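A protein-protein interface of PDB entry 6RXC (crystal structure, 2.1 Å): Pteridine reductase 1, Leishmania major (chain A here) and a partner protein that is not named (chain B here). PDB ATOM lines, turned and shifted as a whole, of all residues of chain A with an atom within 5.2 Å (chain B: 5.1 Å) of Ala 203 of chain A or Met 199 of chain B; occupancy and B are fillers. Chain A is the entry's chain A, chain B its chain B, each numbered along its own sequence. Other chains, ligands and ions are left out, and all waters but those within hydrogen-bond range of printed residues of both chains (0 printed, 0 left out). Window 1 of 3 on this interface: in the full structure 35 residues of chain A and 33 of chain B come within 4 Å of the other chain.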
ATOM      1  N   ALA A 151       9.079  32.682 -27.483  1.00  0.00           N
ATOM      2  CA  ALA A 151      10.206  31.751 -27.555  1.00  0.00           C
ATOM      3  C   ALA A 151      11.498  32.334 -27.032  1.00  0.00           C
ATOM      4  O   ALA A 151      12.133  31.754 -26.137  1.00  0.00           O
ATOM      5  CB  ALA A 151      10.393  31.108 -28.927  1.00  0.00           C
ATOM      6  N   ILE A 152      11.876  33.518 -27.537  1.00  0.00           N
ATOM      7  CA  ILE A 152      13.223  33.952 -27.155  1.00  0.00           C
ATOM      8  C   ILE A 152      13.186  34.506 -25.745  1.00  0.00           C
ATOM      9  O   ILE A 152      14.155  34.321 -25.004  1.00  0.00           O
ATOM     10  CB  ILE A 152      13.767  35.005 -28.137  1.00  0.00           C
ATOM     11  CG1 ILE A 152      13.818  34.425 -29.560  1.00  0.00           C
ATOM     12  CG2 ILE A 152      15.088  35.578 -27.639  1.00  0.00           C
ATOM     13  CD1 ILE A 152      13.756  35.501 -30.611  1.00  0.00           C
ATOM     14  N   TYR A 155      13.488  31.713 -23.478  1.00  0.00           N
ATOM     15  CA  TYR A 155      14.858  31.226 -23.410  1.00  0.00           C
ATOM     16  C   TYR A 155      15.608  32.042 -22.375  1.00  0.00           C
ATOM     17  O   TYR A 155      16.304  31.464 -21.526  1.00  0.00           O
ATOM     18  CB  TYR A 155      15.548  31.314 -24.793  1.00  0.00           C
ATOM     19  CG  TYR A 155      17.021  30.963 -24.729  1.00  0.00           C
ATOM     20  CD1 TYR A 155      17.419  29.652 -24.570  1.00  0.00           C
ATOM     21  CD2 TYR A 155      18.010  31.951 -24.702  1.00  0.00           C
ATOM     22  CE1 TYR A 155      18.760  29.324 -24.402  1.00  0.00           C
ATOM     23  CE2 TYR A 155      19.360  31.626 -24.601  1.00  0.00           C
ATOM     24  CZ  TYR A 155      19.732  30.304 -24.435  1.00  0.00           C
ATOM     25  OH  TYR A 155      21.021  29.920 -24.254  1.00  0.00           O
ATOM     26  N   MET A 199       5.262  28.623 -35.377  1.00  0.00           N
ATOM     27  CA  MET A 199       6.709  28.357 -35.336  1.00  0.00           C
ATOM     28  C   MET A 199       7.274  28.624 -33.937  1.00  0.00           C
ATOM     29  O   MET A 199       8.187  27.949 -33.429  1.00  0.00           O
ATOM     30  CB  MET A 199       7.418  29.296 -36.325  1.00  0.00           C
ATOM     31  CG  MET A 199       7.256  28.850 -37.770  1.00  0.00           C
ATOM     32  SD  MET A 199       8.101  30.017 -38.889  1.00  0.00           S
ATOM     33  CE  MET A 199       9.785  29.360 -38.621  1.00  0.00           C
ATOM     34  N   ALA A 200       6.836  29.748 -33.376  1.00  0.00           N
ATOM     35  CA  ALA A 200       7.387  30.179 -32.095  1.00  0.00           C
ATOM     36  C   ALA A 200       6.957  29.167 -31.007  1.00  0.00           C
ATOM     37  O   ALA A 200       7.777  28.794 -30.183  1.00  0.00           O
ATOM     38  CB  ALA A 200       6.886  31.562 -31.795  1.00  0.00           C
ATOM     39  N   LYS A 201       5.707  28.668 -31.088  1.00  0.00           N
ATOM     40  CA  LYS A 201       5.260  27.595 -30.179  1.00  0.00           C
ATOM     41  C   LYS A 201       6.073  26.320 -30.420  1.00  0.00           C
ATOM     42  O   LYS A 201       6.411  25.578 -29.482  1.00  0.00           O
ATOM     43  CB  LYS A 201       3.749  27.348 -30.247  1.00  0.00           C
ATOM     44  CG  LYS A 201       2.899  28.497 -29.664  1.00  0.00           C
ATOM     45  CD  LYS A 201       3.269  28.877 -28.216  1.00  0.00           C
ATOM     46  CE  LYS A 201       2.059  29.246 -27.364  1.00  0.00           C
ATOM     47  NZ  LYS A 201       2.452  30.002 -26.143  1.00  0.00           N
ATOM     48  N   GLY A 202       6.493  26.125 -31.670  1.00  0.00           N
ATOM     49  CA  GLY A 202       7.249  24.898 -31.868  1.00  0.00           C
ATOM     50  C   GLY A 202       8.650  25.030 -31.307  1.00  0.00           C
ATOM     51  O   GLY A 202       9.201  24.048 -30.849  1.00  0.00           O
ATOM     52  N   ALA A 203       9.232  26.230 -31.444  1.00  0.00           N
ATOM     53  CA  ALA A 203      10.405  26.668 -30.690  1.00  0.00           C
ATOM     54  C   ALA A 203      10.267  26.438 -29.171  1.00  0.00           C
ATOM     55  O   ALA A 203      11.216  26.016 -28.502  1.00  0.00           O
ATOM     56  CB  ALA A 203      10.646  28.122 -31.017  1.00  0.00           C
ATOM     57  N   LEU A 204       9.133  26.873 -28.595  1.00  0.00           N
ATOM     58  CA  LEU A 204       8.939  26.785 -27.141  1.00  0.00           C
ATOM     59  C   LEU A 204       8.960  25.333 -26.689  1.00  0.00           C
ATOM     60  O   LEU A 204       9.545  25.026 -25.653  1.00  0.00           O
ATOM     61  CB  LEU A 204       7.636  27.472 -26.761  1.00  0.00           C
ATOM     62  CG  LEU A 204       7.395  27.599 -25.259  1.00  0.00           C
ATOM     63  CD1 LEU A 204       8.634  28.085 -24.518  1.00  0.00           C
ATOM     64  CD2 LEU A 204       6.110  28.419 -24.959  1.00  0.00           C
ATOM     65  N   GLU A 205       8.466  24.442 -27.557  1.00  0.00           N
ATOM     66  CA  GLU A 205       8.512  23.019 -27.236  1.00  0.00           C
ATOM     67  C   GLU A 205       9.962  22.515 -27.203  1.00  0.00           C
ATOM     68  O   GLU A 205      10.289  21.685 -26.369  1.00  0.00           O
ATOM     69  CB  GLU A 205       7.689  22.192 -28.230  1.00  0.00           C
ATOM     70  CG  GLU A 205       6.193  22.270 -27.983  1.00  0.00           C
ATOM     71  CD  GLU A 205       5.482  21.568 -29.142  1.00  0.00           C
ATOM     72  OE1 GLU A 205       5.797  20.375 -29.352  1.00  0.00           O
ATOM     73  OE2 GLU A 205       4.681  22.224 -29.883  1.00  0.00           O
ATOM     74  N   GLY A 206      10.847  23.048 -28.071  1.00  0.00           N
ATOM     75  CA  GLY A 206      12.219  22.551 -28.061  1.00  0.00           C
ATOM     76  C   GLY A 206      12.969  23.096 -26.855  1.00  0.00           C
ATOM     77  O   GLY A 206      13.850  22.459 -26.296  1.00  0.00           O
ATOM     78  N   LEU A 207      12.716  24.377 -26.515  1.00  0.00           N
ATOM     79  CA  LEU A 207      13.319  24.903 -25.305  1.00  0.00           C
ATOM     80  C   LEU A 207      12.870  24.036 -24.103  1.00  0.00           C
ATOM     81  O   LEU A 207      13.706  23.608 -23.290  1.00  0.00           O
ATOM     82  CB  LEU A 207      12.813  26.339 -25.172  1.00  0.00           C
ATOM     83  CG  LEU A 207      13.030  26.996 -23.804  1.00  0.00           C
ATOM     84  CD1 LEU A 207      14.499  27.082 -23.527  1.00  0.00           C
ATOM     85  CD2 LEU A 207      12.392  28.404 -23.776  1.00  0.00           C
ATOM     86  N   THR A 208      11.552  23.803 -23.954  1.00  0.00           N
ATOM     87  CA  THR A 208      11.083  22.863 -22.902  1.00  0.00           C
ATOM     88  C   THR A 208      11.962  21.602 -22.868  1.00  0.00           C
ATOM     89  O   THR A 208      12.427  21.161 -21.815  1.00  0.00           O
ATOM     90  CB  THR A 208       9.619  22.431 -23.140  1.00  0.00           C
ATOM     91  OG1 THR A 208       8.690  23.517 -23.102  1.00  0.00           O
ATOM     92  CG2 THR A 208       9.103  21.514 -22.043  1.00  0.00           C
ATOM     93  N   PHE B 147      18.576  31.465 -35.128  1.00  0.00           N
ATOM     94  CA  PHE B 147      17.165  31.588 -35.540  1.00  0.00           C
ATOM     95  C   PHE B 147      16.953  32.150 -36.947  1.00  0.00           C
ATOM     96  O   PHE B 147      16.096  31.652 -37.668  1.00  0.00           O
ATOM     97  CB  PHE B 147      16.411  32.524 -34.603  1.00  0.00           C
ATOM     98  CG  PHE B 147      15.955  31.800 -33.366  1.00  0.00           C
ATOM     99  CD1 PHE B 147      14.975  30.822 -33.452  1.00  0.00           C
ATOM    100  CD2 PHE B 147      16.573  32.034 -32.147  1.00  0.00           C
ATOM    101  CE1 PHE B 147      14.583  30.099 -32.334  1.00  0.00           C
ATOM    102  CE2 PHE B 147      16.187  31.308 -31.027  1.00  0.00           C
ATOM    103  CZ  PHE B 147      15.201  30.333 -31.126  1.00  0.00           C
ATOM    104  N   TYR B 194      22.734  23.026 -26.653  1.00  0.00           N
ATOM    105  CA  TYR B 194      22.382  23.483 -27.980  1.00  0.00           C
ATOM    106  C   TYR B 194      20.966  24.078 -28.064  1.00  0.00           C
ATOM    107  O   TYR B 194      20.279  23.919 -29.093  1.00  0.00           O
ATOM    108  CB  TYR B 194      22.703  22.430 -29.036  1.00  0.00           C
ATOM    109  CG  TYR B 194      24.167  22.191 -29.355  1.00  0.00           C
ATOM    110  CD1 TYR B 194      24.973  21.376 -28.560  1.00  0.00           C
ATOM    111  CD2 TYR B 194      24.743  22.776 -30.479  1.00  0.00           C
ATOM    112  CE1 TYR B 194      26.301  21.130 -28.872  1.00  0.00           C
ATOM    113  CE2 TYR B 194      26.080  22.560 -30.785  1.00  0.00           C
ATOM    114  CZ  TYR B 194      26.849  21.734 -29.989  1.00  0.00           C
ATOM    115  OH  TYR B 194      28.138  21.489 -30.347  1.00  0.00           O
ATOM    116  N   THR B 195      20.434  24.636 -26.962  1.00  0.00           N
ATOM    117  CA  THR B 195      18.992  25.059 -26.931  1.00  0.00           C
ATOM    118  C   THR B 195      18.565  25.933 -28.109  1.00  0.00           C
ATOM    119  O   THR B 195      17.512  25.618 -28.701  1.00  0.00           O
ATOM    120  CB  THR B 195      18.551  25.839 -25.685  1.00  0.00           C
ATOM    121  OG1 THR B 195      18.878  25.057 -24.535  1.00  0.00           O
ATOM    122  CG2 THR B 195      17.072  26.160 -25.684  1.00  0.00           C
ATOM    123  N   ILE B 196      19.302  27.022 -28.364  1.00  0.00           N
ATOM    124  CA  ILE B 196      18.984  27.967 -29.476  1.00  0.00           C
ATOM    125  C   ILE B 196      18.753  27.145 -30.746  1.00  0.00           C
ATOM    126  O   ILE B 196      17.655  27.243 -31.329  1.00  0.00           O
ATOM    127  CB  ILE B 196      20.113  29.000 -29.659  1.00  0.00           C
ATOM    128  CG1 ILE B 196      20.409  29.755 -28.360  1.00  0.00           C
ATOM    129  CG2 ILE B 196      19.796  29.950 -30.804  1.00  0.00           C
ATOM    130  CD1 ILE B 196      19.883  31.170 -28.338  1.00  0.00           C
ATOM    131  N   TYR B 197      19.762  26.366 -31.144  1.00  0.00           N
ATOM    132  CA  TYR B 197      19.652  25.508 -32.314  1.00  0.00           C
ATOM    133  C   TYR B 197      18.382  24.617 -32.199  1.00  0.00           C
ATOM    134  O   TYR B 197      17.673  24.382 -33.170  1.00  0.00           O
ATOM    135  CB  TYR B 197      20.994  24.730 -32.498  1.00  0.00           C
ATOM    136  CG  TYR B 197      20.908  23.599 -33.495  1.00  0.00           C
ATOM    137  CD1 TYR B 197      20.949  23.826 -34.871  1.00  0.00           C
ATOM    138  CD2 TYR B 197      20.632  22.314 -33.070  1.00  0.00           C
ATOM    139  CE1 TYR B 197      20.798  22.787 -35.768  1.00  0.00           C
ATOM    140  CE2 TYR B 197      20.554  21.253 -33.947  1.00  0.00           C
ATOM    141  CZ  TYR B 197      20.576  21.498 -35.302  1.00  0.00           C
ATOM    142  OH  TYR B 197      20.389  20.424 -36.116  1.00  0.00           O
ATOM    143  N   THR B 198      18.147  23.965 -31.049  1.00  0.00           N
ATOM    144  CA  THR B 198      17.096  22.962 -30.990  1.00  0.00           C
ATOM    145  C   THR B 198      15.754  23.676 -31.130  1.00  0.00           C
ATOM    146  O   THR B 198      14.840  23.153 -31.723  1.00  0.00           O
ATOM    147  CB  THR B 198      17.212  22.243 -29.651  1.00  0.00           C
ATOM    148  OG1 THR B 198      18.414  21.464 -29.761  1.00  0.00           O
ATOM    149  CG2 THR B 198      16.031  21.348 -29.290  1.00  0.00           C
ATOM    150  N   MET B 199      15.665  24.901 -30.579  1.00  0.00           N
ATOM    151  CA  MET B 199      14.442  25.656 -30.698  1.00  0.00           C
ATOM    152  C   MET B 199      14.192  26.036 -32.165  1.00  0.00           C
ATOM    153  O   MET B 199      13.014  26.138 -32.609  1.00  0.00           O
ATOM    154  CB  MET B 199      14.529  26.946 -29.870  1.00  0.00           C
ATOM    155  CG  MET B 199      14.495  26.724 -28.344  1.00  0.00           C
ATOM    156  SD  MET B 199      14.764  28.252 -27.463  1.00  0.00           S
ATOM    157  CE  MET B 199      13.295  29.206 -27.813  1.00  0.00           C
ATOM    158  N   ALA B 200      15.294  26.343 -32.882  1.00  0.00           N
ATOM    159  CA  ALA B 200      15.146  26.898 -34.231  1.00  0.00           C
ATOM    160  C   ALA B 200      14.649  25.787 -35.173  1.00  0.00           C
ATOM    161  O   ALA B 200      13.785  26.051 -36.010  1.00  0.00           O
ATOM    162  CB  ALA B 200      16.482  27.551 -34.646  1.00  0.00           C
ATOM    163  N   LYS B 201      15.150  24.555 -34.999  1.00  0.00           N
ATOM    164  CA  LYS B 201      14.683  23.327 -35.667  1.00  0.00           C
ATOM    165  C   LYS B 201      13.218  22.972 -35.382  1.00  0.00           C
ATOM    166  O   LYS B 201      12.441  22.651 -36.298  1.00  0.00           O
ATOM    167  CB  LYS B 201      15.564  22.125 -35.249  1.00  0.00           C
ATOM    168  CG  LYS B 201      16.916  22.054 -35.986  1.00  0.00           C
ATOM    169  CD  LYS B 201      16.873  22.473 -37.485  1.00  0.00           C
ATOM    170  CE  LYS B 201      18.197  22.194 -38.212  1.00  0.00           C
ATOM    171  NZ  LYS B 201      18.295  22.745 -39.588  1.00  0.00           N
ATOM    172  N   GLY B 202      12.774  23.208 -34.132  1.00  0.00           N
ATOM    173  CA  GLY B 202      11.349  23.025 -33.808  1.00  0.00           C
ATOM    174  C   GLY B 202      10.439  24.081 -34.446  1.00  0.00           C
ATOM    175  O   GLY B 202       9.353  23.706 -34.946  1.00  0.00           O
ATOM    176  N   ALA B 203      10.967  25.331 -34.618  1.00  0.00           N
ATOM    177  CA  ALA B 203      10.268  26.361 -35.398  1.00  0.00           C
ATOM    178  C   ALA B 203      10.158  25.937 -36.860  1.00  0.00           C
ATOM    179  O   ALA B 203       9.076  26.059 -37.465  1.00  0.00           O
ATOM    180  CB  ALA B 203      10.914  27.726 -35.304  1.00  0.00           C
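The side-chain hydroxyl (OG1) of Thr 198 of chain B is in hydrogen-bond range of the backbone carbonyl oxygen (O) of Tyr 194 of chain B (3.2 Å).
Among the printed residues, merely in contact across the chains: Ala 151 of chain A with Met 199 of chain B, Met 199 of chain A with Ala 203 of chain B, Ala 203 of chain A with Met 199 of chain B, Leu 207 of chain A with Met 199 of chain B, Leu 207 of chain A with Thr 195 of chain B, Tyr 155 of chain A with Thr 195 of chain B, Ala 203 of chain A with Ala 203 of chain B, Gly 202 of chain A with Gly 202 of chain B, Tyr 155 of chain A with Ile 196 of chain B, Gly 206 of chain A with Thr 198 of chain B and Ala 203 of chain A with Gly 202 of chain B.
Lys 201 of chain A touches none of the printed residues of chain B.
Of chain B, only Met 199, Gly 202 and Ala 203 come within 4 Å of Ala 203 of chain A.
Of the printed residues of chain B, Gly 206 of chain A touches Thr 198.
Of the printed residues of chain A, Thr 195 of chain B touches Tyr 155 (3.7 Å) and Leu 207 (3.5 Å).
Of the printed residues of chain A, Thr 198 of chain B touches Gly 206 (3.9 Å).
Of chain A, only Ala 151, Ala 203 and Leu 207 come within 4 Å of Met 199 of chain B.
Of the printed residues of chain A, Ala 203 of chain B touches Met 199 and Ala 203.
The nearest residue of chain B that does not touch Ala 203 of chain A is Phe 147 of chain B (4.6 Å).
The nearest residue of chain A that does not touch Met 199 of chain B is Tyr 155 of chain A (4.1 Å).
The nearest printed residue of chain B that does not touch Tyr 155 of chain A is Met 199 of chain B (4.1 Å).
Of the 13 printed residues of chain A, 7 touch a printed residue of chain B.
Printed residues of chain A that touch a printed residue of chain B: Ala 151, Tyr 155, Met 199, Gly 202, Ala 203, Gly 206 and Leu 207.
Hydrophobic or aromatic side chains of chain A within 4 Å of the printed part of chain B: Ala 151, Tyr 155, Met 199, Ala 203 and Leu 207.
Hydrophobic or aromatic side chains of chain B that line the printed part of chain A: Ile 196, Met 199 and Ala 203.
Among the printed residues, 11 pairs touch across the chains.
Among the printed residues, no Asp or Glu carboxylate lies within 4 Å of a Lys or Arg side-chain nitrogen of the other chain.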
